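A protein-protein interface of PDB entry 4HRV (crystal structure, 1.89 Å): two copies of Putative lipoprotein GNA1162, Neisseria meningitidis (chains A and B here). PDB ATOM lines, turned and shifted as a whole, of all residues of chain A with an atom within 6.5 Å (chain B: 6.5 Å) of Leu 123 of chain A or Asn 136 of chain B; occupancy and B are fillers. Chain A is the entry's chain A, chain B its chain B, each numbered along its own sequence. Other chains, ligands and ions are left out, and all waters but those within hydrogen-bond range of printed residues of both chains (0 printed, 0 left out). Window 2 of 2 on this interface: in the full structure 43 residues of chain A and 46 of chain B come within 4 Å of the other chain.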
ATOM      1  N   PRO A  13      13.440 -13.500 -10.873  1.00  0.00           N
ATOM      2  CA  PRO A  13      13.569 -12.095 -11.271  1.00  0.00           C
ATOM      3  C   PRO A  13      12.386 -11.672 -12.122  1.00  0.00           C
ATOM      4  O   PRO A  13      12.374 -11.919 -13.324  1.00  0.00           O
ATOM      5  CB  PRO A  13      14.848 -12.082 -12.121  1.00  0.00           C
ATOM      6  CG  PRO A  13      15.297 -13.544 -12.237  1.00  0.00           C
ATOM      7  CD  PRO A  13      14.138 -14.387 -11.813  1.00  0.00           C
ATOM      8  N   ASP A  85      13.981  -6.240  -9.120  1.00  0.00           N
ATOM      9  CA  ASP A  85      14.630  -7.495  -8.747  1.00  0.00           C
ATOM     10  C   ASP A  85      16.058  -7.535  -9.274  1.00  0.00           C
ATOM     11  O   ASP A  85      16.967  -8.031  -8.594  1.00  0.00           O
ATOM     12  CB  ASP A  85      13.863  -8.691  -9.317  1.00  0.00           C
ATOM     13  CG  ASP A  85      12.504  -8.878  -8.670  1.00  0.00           C
ATOM     14  OD1 ASP A  85      11.562  -9.289  -9.382  1.00  0.00           O
ATOM     15  OD2 ASP A  85      12.387  -8.631  -7.451  1.00  0.00           O
ATOM     16  N   ALA A  86      16.253  -7.007 -10.486  1.00  0.00           N
ATOM     17  CA  ALA A  86      17.527  -7.152 -11.182  1.00  0.00           C
ATOM     18  C   ALA A  86      17.922  -5.926 -12.000  1.00  0.00           C
ATOM     19  O   ALA A  86      17.107  -5.043 -12.282  1.00  0.00           O
ATOM     20  CB  ALA A  86      17.487  -8.368 -12.079  1.00  0.00           C
ATOM     21  N   VAL A  87      19.178  -5.902 -12.413  1.00  0.00           N
ATOM     22  CA  VAL A  87      19.703  -4.799 -13.197  1.00  0.00           C
ATOM     23  C   VAL A  87      20.438  -5.367 -14.389  1.00  0.00           C
ATOM     24  O   VAL A  87      21.276  -6.265 -14.232  1.00  0.00           O
ATOM     25  CB  VAL A  87      20.698  -3.967 -12.376  1.00  0.00           C
ATOM     26  CG1 VAL A  87      21.097  -2.704 -13.136  1.00  0.00           C
ATOM     27  CG2 VAL A  87      20.116  -3.635 -11.031  1.00  0.00           C
ATOM     28  N   ARG A 113      25.362  -8.380 -18.639  1.00  0.00           N
ATOM     29  CA  ARG A 113      25.176  -9.224 -17.482  1.00  0.00           C
ATOM     30  C   ARG A 113      23.930  -8.788 -16.743  1.00  0.00           C
ATOM     31  O   ARG A 113      23.624  -7.605 -16.657  1.00  0.00           O
ATOM     32  CB  ARG A 113      26.404  -9.163 -16.571  1.00  0.00           C
ATOM     33  CG  ARG A 113      26.764  -7.775 -16.093  1.00  0.00           C
ATOM     34  CD  ARG A 113      28.124  -7.805 -15.387  1.00  0.00           C
ATOM     35  NE  ARG A 113      28.098  -7.037 -14.147  1.00  0.00           N
ATOM     36  CZ  ARG A 113      28.375  -5.743 -14.071  1.00  0.00           C
ATOM     37  NH1 ARG A 113      28.708  -5.065 -15.158  1.00  0.00           N
ATOM     38  NH2 ARG A 113      28.329  -5.132 -12.906  1.00  0.00           N
ATOM     39  N   LEU A 114      23.189  -9.758 -16.239  1.00  0.00           N
ATOM     40  CA  LEU A 114      22.009  -9.458 -15.456  1.00  0.00           C
ATOM     41  C   LEU A 114      22.407  -9.744 -14.020  1.00  0.00           C
ATOM     42  O   LEU A 114      22.941 -10.815 -13.726  1.00  0.00           O
ATOM     43  CB  LEU A 114      20.841 -10.358 -15.866  1.00  0.00           C
ATOM     44  CG  LEU A 114      19.527 -10.066 -15.135  1.00  0.00           C
ATOM     45  CD1 LEU A 114      19.006  -8.691 -15.572  1.00  0.00           C
ATOM     46  CD2 LEU A 114      18.497 -11.144 -15.409  1.00  0.00           C
ATOM     47  N   VAL A 115      22.175  -8.773 -13.143  1.00  0.00           N
ATOM     48  CA  VAL A 115      22.629  -8.850 -11.764  1.00  0.00           C
ATOM     49  C   VAL A 115      21.470  -8.726 -10.768  1.00  0.00           C
ATOM     50  O   VAL A 115      20.613  -7.836 -10.897  1.00  0.00           O
ATOM     51  CB  VAL A 115      23.668  -7.741 -11.484  1.00  0.00           C
ATOM     52  CG1 VAL A 115      23.975  -7.641 -10.022  1.00  0.00           C
ATOM     53  CG2 VAL A 115      24.951  -8.000 -12.287  1.00  0.00           C
ATOM     54  N   ASP A 116      21.437  -9.627  -9.786  1.00  0.00           N
ATOM     55  CA  ASP A 116      20.439  -9.567  -8.733  1.00  0.00           C
ATOM     56  C   ASP A 116      20.664  -8.269  -7.949  1.00  0.00           C
ATOM     57  O   ASP A 116      21.756  -8.013  -7.457  1.00  0.00           O
ATOM     58  CB  ASP A 116      20.549 -10.807  -7.827  1.00  0.00           C
ATOM     59  CG  ASP A 116      19.595 -10.765  -6.640  1.00  0.00           C
ATOM     60  OD1 ASP A 116      19.528  -9.720  -5.963  1.00  0.00           O
ATOM     61  OD2 ASP A 116      18.918 -11.788  -6.376  1.00  0.00           O
ATOM     62  N   SER A 117      19.635  -7.434  -7.866  1.00  0.00           N
ATOM     63  CA  SER A 117      19.825  -6.080  -7.366  1.00  0.00           C
ATOM     64  C   SER A 117      19.970  -6.020  -5.833  1.00  0.00           C
ATOM     65  O   SER A 117      20.493  -5.047  -5.287  1.00  0.00           O
ATOM     66  CB  SER A 117      18.685  -5.170  -7.849  1.00  0.00           C
ATOM     67  OG  SER A 117      19.083  -3.812  -7.812  1.00  0.00           O
ATOM     68  N   ASN A 119      21.703  -8.424  -3.837  1.00  0.00           N
ATOM     69  CA  ASN A 119      22.998  -8.928  -3.365  1.00  0.00           C
ATOM     70  C   ASN A 119      24.140  -8.758  -4.359  1.00  0.00           C
ATOM     71  O   ASN A 119      25.304  -9.067  -4.059  1.00  0.00           O
ATOM     72  CB  ASN A 119      22.889 -10.396  -2.925  1.00  0.00           C
ATOM     73  CG  ASN A 119      22.215 -11.278  -3.970  1.00  0.00           C
ATOM     74  OD1 ASN A 119      21.460 -12.195  -3.638  1.00  0.00           O
ATOM     75  ND2 ASN A 119      22.468 -10.993  -5.234  1.00  0.00           N
ATOM     76  N   LYS A 121      24.620 -10.458  -6.938  1.00  0.00           N
ATOM     77  CA  LYS A 121      24.951 -11.752  -7.541  1.00  0.00           C
ATOM     78  C   LYS A 121      24.654 -11.750  -9.031  1.00  0.00           C
ATOM     79  O   LYS A 121      23.605 -11.272  -9.464  1.00  0.00           O
ATOM     80  CB  LYS A 121      24.151 -12.871  -6.868  1.00  0.00           C
ATOM     81  CG  LYS A 121      24.432 -14.263  -7.411  1.00  0.00           C
ATOM     82  CD  LYS A 121      23.900 -15.330  -6.465  1.00  0.00           C
ATOM     83  CE  LYS A 121      24.144 -16.734  -7.012  1.00  0.00           C
ATOM     84  NZ  LYS A 121      23.644 -17.783  -6.062  1.00  0.00           N
ATOM     85  N   GLU A 122      25.564 -12.305  -9.820  1.00  0.00           N
ATOM     86  CA  GLU A 122      25.325 -12.375 -11.256  1.00  0.00           C
ATOM     87  C   GLU A 122      24.323 -13.484 -11.602  1.00  0.00           C
ATOM     88  O   GLU A 122      24.439 -14.615 -11.133  1.00  0.00           O
ATOM     89  CB  GLU A 122      26.622 -12.572 -12.008  1.00  0.00           C
ATOM     90  CG  GLU A 122      26.461 -12.497 -13.517  1.00  0.00           C
ATOM     91  CD  GLU A 122      27.786 -12.573 -14.218  1.00  0.00           C
ATOM     92  OE1 GLU A 122      28.106 -13.659 -14.734  1.00  0.00           O
ATOM     93  OE2 GLU A 122      28.510 -11.553 -14.239  1.00  0.00           O
ATOM     94  N   LEU A 123      23.329 -13.142 -12.412  1.00  0.00           N
ATOM     95  CA  LEU A 123      22.255 -14.078 -12.754  1.00  0.00           C
ATOM     96  C   LEU A 123      22.435 -14.629 -14.159  1.00  0.00           C
ATOM     97  O   LEU A 123      22.054 -15.765 -14.456  1.00  0.00           O
ATOM     98  CB  LEU A 123      20.896 -13.370 -12.666  1.00  0.00           C
ATOM     99  CG  LEU A 123      20.542 -12.871 -11.263  1.00  0.00           C
ATOM    100  CD1 LEU A 123      19.292 -11.991 -11.315  1.00  0.00           C
ATOM    101  CD2 LEU A 123      20.354 -14.051 -10.319  1.00  0.00           C
ATOM    102  N   TRP A 124      23.016 -13.810 -15.027  1.00  0.00           N
ATOM    103  CA  TRP A 124      23.222 -14.204 -16.412  1.00  0.00           C
ATOM    104  C   TRP A 124      24.297 -13.334 -17.044  1.00  0.00           C
ATOM    105  O   TRP A 124      24.484 -12.165 -16.679  1.00  0.00           O
ATOM    106  CB  TRP A 124      21.910 -14.073 -17.202  1.00  0.00           C
ATOM    107  CG  TRP A 124      22.070 -14.269 -18.673  1.00  0.00           C
ATOM    108  CD1 TRP A 124      22.050 -15.460 -19.352  1.00  0.00           C
ATOM    109  CD2 TRP A 124      22.272 -13.249 -19.659  1.00  0.00           C
ATOM    110  NE1 TRP A 124      22.222 -15.237 -20.701  1.00  0.00           N
ATOM    111  CE2 TRP A 124      22.363 -13.890 -20.915  1.00  0.00           C
ATOM    112  CE3 TRP A 124      22.384 -11.855 -19.605  1.00  0.00           C
ATOM    113  CZ2 TRP A 124      22.571 -13.188 -22.098  1.00  0.00           C
ATOM    114  CZ3 TRP A 124      22.585 -11.159 -20.794  1.00  0.00           C
ATOM    115  CH2 TRP A 124      22.668 -11.827 -22.019  1.00  0.00           C
ATOM    116  N   SER A 125      25.003 -13.921 -17.994  1.00  0.00           N
ATOM    117  CA  SER A 125      26.100 -13.256 -18.665  1.00  0.00           C
ATOM    118  C   SER A 125      26.113 -13.720 -20.126  1.00  0.00           C
ATOM    119  O   SER A 125      25.879 -14.890 -20.405  1.00  0.00           O
ATOM    120  CB  SER A 125      27.400 -13.666 -17.965  1.00  0.00           C
ATOM    121  OG  SER A 125      28.510 -12.966 -18.473  1.00  0.00           O
ATOM    122  N   ASP B 103      33.157 -21.755 -14.236  1.00  0.00           N
ATOM    123  CA  ASP B 103      32.064 -21.761 -15.196  1.00  0.00           C
ATOM    124  C   ASP B 103      32.584 -22.143 -16.573  1.00  0.00           C
ATOM    125  O   ASP B 103      33.754 -21.936 -16.890  1.00  0.00           O
ATOM    126  CB  ASP B 103      31.377 -20.392 -15.252  1.00  0.00           C
ATOM    127  CG  ASP B 103      30.103 -20.412 -16.081  1.00  0.00           C
ATOM    128  OD1 ASP B 103      29.588 -21.520 -16.352  1.00  0.00           O
ATOM    129  OD2 ASP B 103      29.615 -19.317 -16.447  1.00  0.00           O
ATOM    130  N   GLU B 132      27.825 -17.369 -24.191  1.00  0.00           N
ATOM    131  CA  GLU B 132      26.985 -17.339 -23.012  1.00  0.00           C
ATOM    132  C   GLU B 132      27.628 -18.137 -21.897  1.00  0.00           C
ATOM    133  O   GLU B 132      28.204 -19.198 -22.139  1.00  0.00           O
ATOM    134  CB  GLU B 132      25.622 -17.922 -23.350  1.00  0.00           C
ATOM    135  CG  GLU B 132      24.549 -17.621 -22.348  1.00  0.00           C
ATOM    136  CD  GLU B 132      23.268 -18.349 -22.668  1.00  0.00           C
ATOM    137  OE1 GLU B 132      23.351 -19.538 -23.054  1.00  0.00           O
ATOM    138  OE2 GLU B 132      22.187 -17.729 -22.551  1.00  0.00           O
ATOM    139  N   GLY B 133      27.542 -17.613 -20.675  1.00  0.00           N
ATOM    140  CA  GLY B 133      27.989 -18.350 -19.508  1.00  0.00           C
ATOM    141  C   GLY B 133      27.156 -19.608 -19.353  1.00  0.00           C
ATOM    142  O   GLY B 133      25.927 -19.545 -19.341  1.00  0.00           O
ATOM    143  N   SER B 134      27.822 -20.753 -19.240  1.00  0.00           N
ATOM    144  CA  SER B 134      27.139 -22.041 -19.161  1.00  0.00           C
ATOM    145  C   SER B 134      26.373 -22.231 -17.848  1.00  0.00           C
ATOM    146  O   SER B 134      25.313 -22.864 -17.822  1.00  0.00           O
ATOM    147  CB  SER B 134      28.134 -23.188 -19.373  1.00  0.00           C
ATOM    148  OG  SER B 134      27.558 -24.443 -19.057  1.00  0.00           O
ATOM    149  N   ASN B 135      26.908 -21.678 -16.765  1.00  0.00           N
ATOM    150  CA  ASN B 135      26.285 -21.802 -15.452  1.00  0.00           C
ATOM    151  C   ASN B 135      24.844 -21.276 -15.392  1.00  0.00           C
ATOM    152  O   ASN B 135      24.032 -21.780 -14.615  1.00  0.00           O
ATOM    153  CB  ASN B 135      27.144 -21.114 -14.388  1.00  0.00           C
ATOM    154  N   ASN B 136      24.522 -20.274 -16.203  1.00  0.00           N
ATOM    155  CA  ASN B 136      23.177 -19.692 -16.177  1.00  0.00           C
ATOM    156  C   ASN B 136      22.554 -19.458 -17.557  1.00  0.00           C
ATOM    157  O   ASN B 136      22.094 -18.350 -17.852  1.00  0.00           O
ATOM    158  CB  ASN B 136      23.171 -18.376 -15.389  1.00  0.00           C
ATOM    159  CG  ASN B 136      23.638 -18.540 -13.950  1.00  0.00           C
ATOM    160  OD1 ASN B 136      22.896 -19.024 -13.093  1.00  0.00           O
ATOM    161  ND2 ASN B 136      24.868 -18.113 -13.673  1.00  0.00           N
ATOM    162  N   SER B 137      22.523 -20.498 -18.389  1.00  0.00           N
ATOM    163  CA  SER B 137      21.986 -20.387 -19.747  1.00  0.00           C
ATOM    164  C   SER B 137      20.570 -19.811 -19.767  1.00  0.00           C
ATOM    165  O   SER B 137      19.760 -20.094 -18.885  1.00  0.00           O
ATOM    166  CB  SER B 137      22.015 -21.748 -20.450  1.00  0.00           C
ATOM    167  N   ASN B 138      20.285 -18.993 -20.774  1.00  0.00           N
ATOM    168  CA  ASN B 138      18.999 -18.309 -20.894  1.00  0.00           C
ATOM    169  C   ASN B 138      18.801 -17.738 -22.306  1.00  0.00           C
ATOM    170  O   ASN B 138      19.357 -16.691 -22.655  1.00  0.00           O
ATOM    171  CB  ASN B 138      18.894 -17.197 -19.838  1.00  0.00           C
ATOM    172  CG  ASN B 138      17.504 -16.578 -19.760  1.00  0.00           C
ATOM    173  OD1 ASN B 138      16.919 -16.473 -18.680  1.00  0.00           O
ATOM    174  ND2 ASN B 138      16.979 -16.155 -20.897  1.00  0.00           N
ATOM    175  N   LEU B 141      17.311 -13.950 -22.626  1.00  0.00           N
ATOM    176  CA  LEU B 141      18.288 -12.878 -22.491  1.00  0.00           C
ATOM    177  C   LEU B 141      19.282 -12.826 -23.649  1.00  0.00           C
ATOM    178  O   LEU B 141      19.642 -11.748 -24.096  1.00  0.00           O
ATOM    179  CB  LEU B 141      19.032 -12.999 -21.149  1.00  0.00           C
ATOM    180  CG  LEU B 141      18.105 -12.908 -19.939  1.00  0.00           C
ATOM    181  CD1 LEU B 141      18.847 -13.157 -18.631  1.00  0.00           C
ATOM    182  CD2 LEU B 141      17.406 -11.547 -19.908  1.00  0.00           C
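Printed residues of chain A within 4 Å of Asn 136 of chain B: Leu 123 and Trp 124.
Of the printed residues of chain A, Leu 141 of chain B touches Leu 114 and Trp 124.
Of the printed residues of chain A, Glu 132 of chain B touches Trp 124 (3.1 Å) and Ser 125 (3.6 Å).
Printed residues of chain B within 4 Å of Trp 124 of chain A: Glu 132, Asn 136, Asn 138 and Leu 141.
Printed residues of chain A within 4 Å of Asn 138 of chain B: Trp 124.
Asn 119 of chain A touches none of the printed residues of chain B.
The nearest residue of chain A that does not touch Asn 136 of chain B is Glu 122 of chain A (4.3 Å).
The nearest printed residue of chain A that does not touch Glu 132 of chain B is Leu 123 of chain A (8.3 Å).
The side-chain amide nitrogen (ND2) of Asn 138 of chain B sits close to the backbone NH (N) of Leu 141 of chain B (2.8 Å).
The backbone carbonyl oxygen of Trp 124 of chain A lies within hydrogen-bond range of the backbone NH of Leu 114 of chain A (2.8 Å).
N of Asn 138 of chain B sits at hydrogen-bond distance from OE2 of Glu 132 of chain B (2.9 Å).
The backbone carbonyl oxygen (O) of Leu 114 of chain A is in hydrogen-bond range of the backbone NH (N) of Leu 123 of chain A (2.7 Å).
Leu 141 of chain B touches Leu 114 of chain A (CD1 to CD2, 3.8 Å).
O of Leu 123 of chain A touches CB of Asn 136 of chain B, 3.0 Å away.
Asn 136 of chain B touches Trp 124 of chain A (O to CD1, 3.3 Å).
Asn 138 of chain B touches Trp 124 of chain A.
CD1 of Leu 141 of chain B touches CG of Trp 124 of chain A, at 3.4 Å.
O of Ser 125 of chain A touches CG of Glu 132 of chain B, 3.6 Å away.
Printed residues of chain A that touch a printed residue of chain B: Leu 114, Leu 123, Trp 124 and Ser 125.
Hydrophobic or aromatic side chains of chain A within 4 Å of the printed part of chain B: Leu 114 and Trp 124.
Among the printed residues, 8 pairs touch across the chains.
Among the printed residues, no Asp or Glu carboxylate lies within 4 Å of a Lys or Arg side-chain nitrogen of the other chain.
The side-chain carboxylate (OE2) of Glu 132 of chain B sits at hydrogen-bond distance from the indole nitrogen (NE1) of Trp 124 of chain A (3.1 Å).
The backbone carbonyl oxygen of Ser 125 of chain A sits at hydrogen-bond distance from the backbone NH of Gly 133 of chain B (3.2 Å).
No position is printed for both chains.
Of the 8 pairs that touch across the chains among the printed residues, none has its exchanged pair printed and touching as well.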
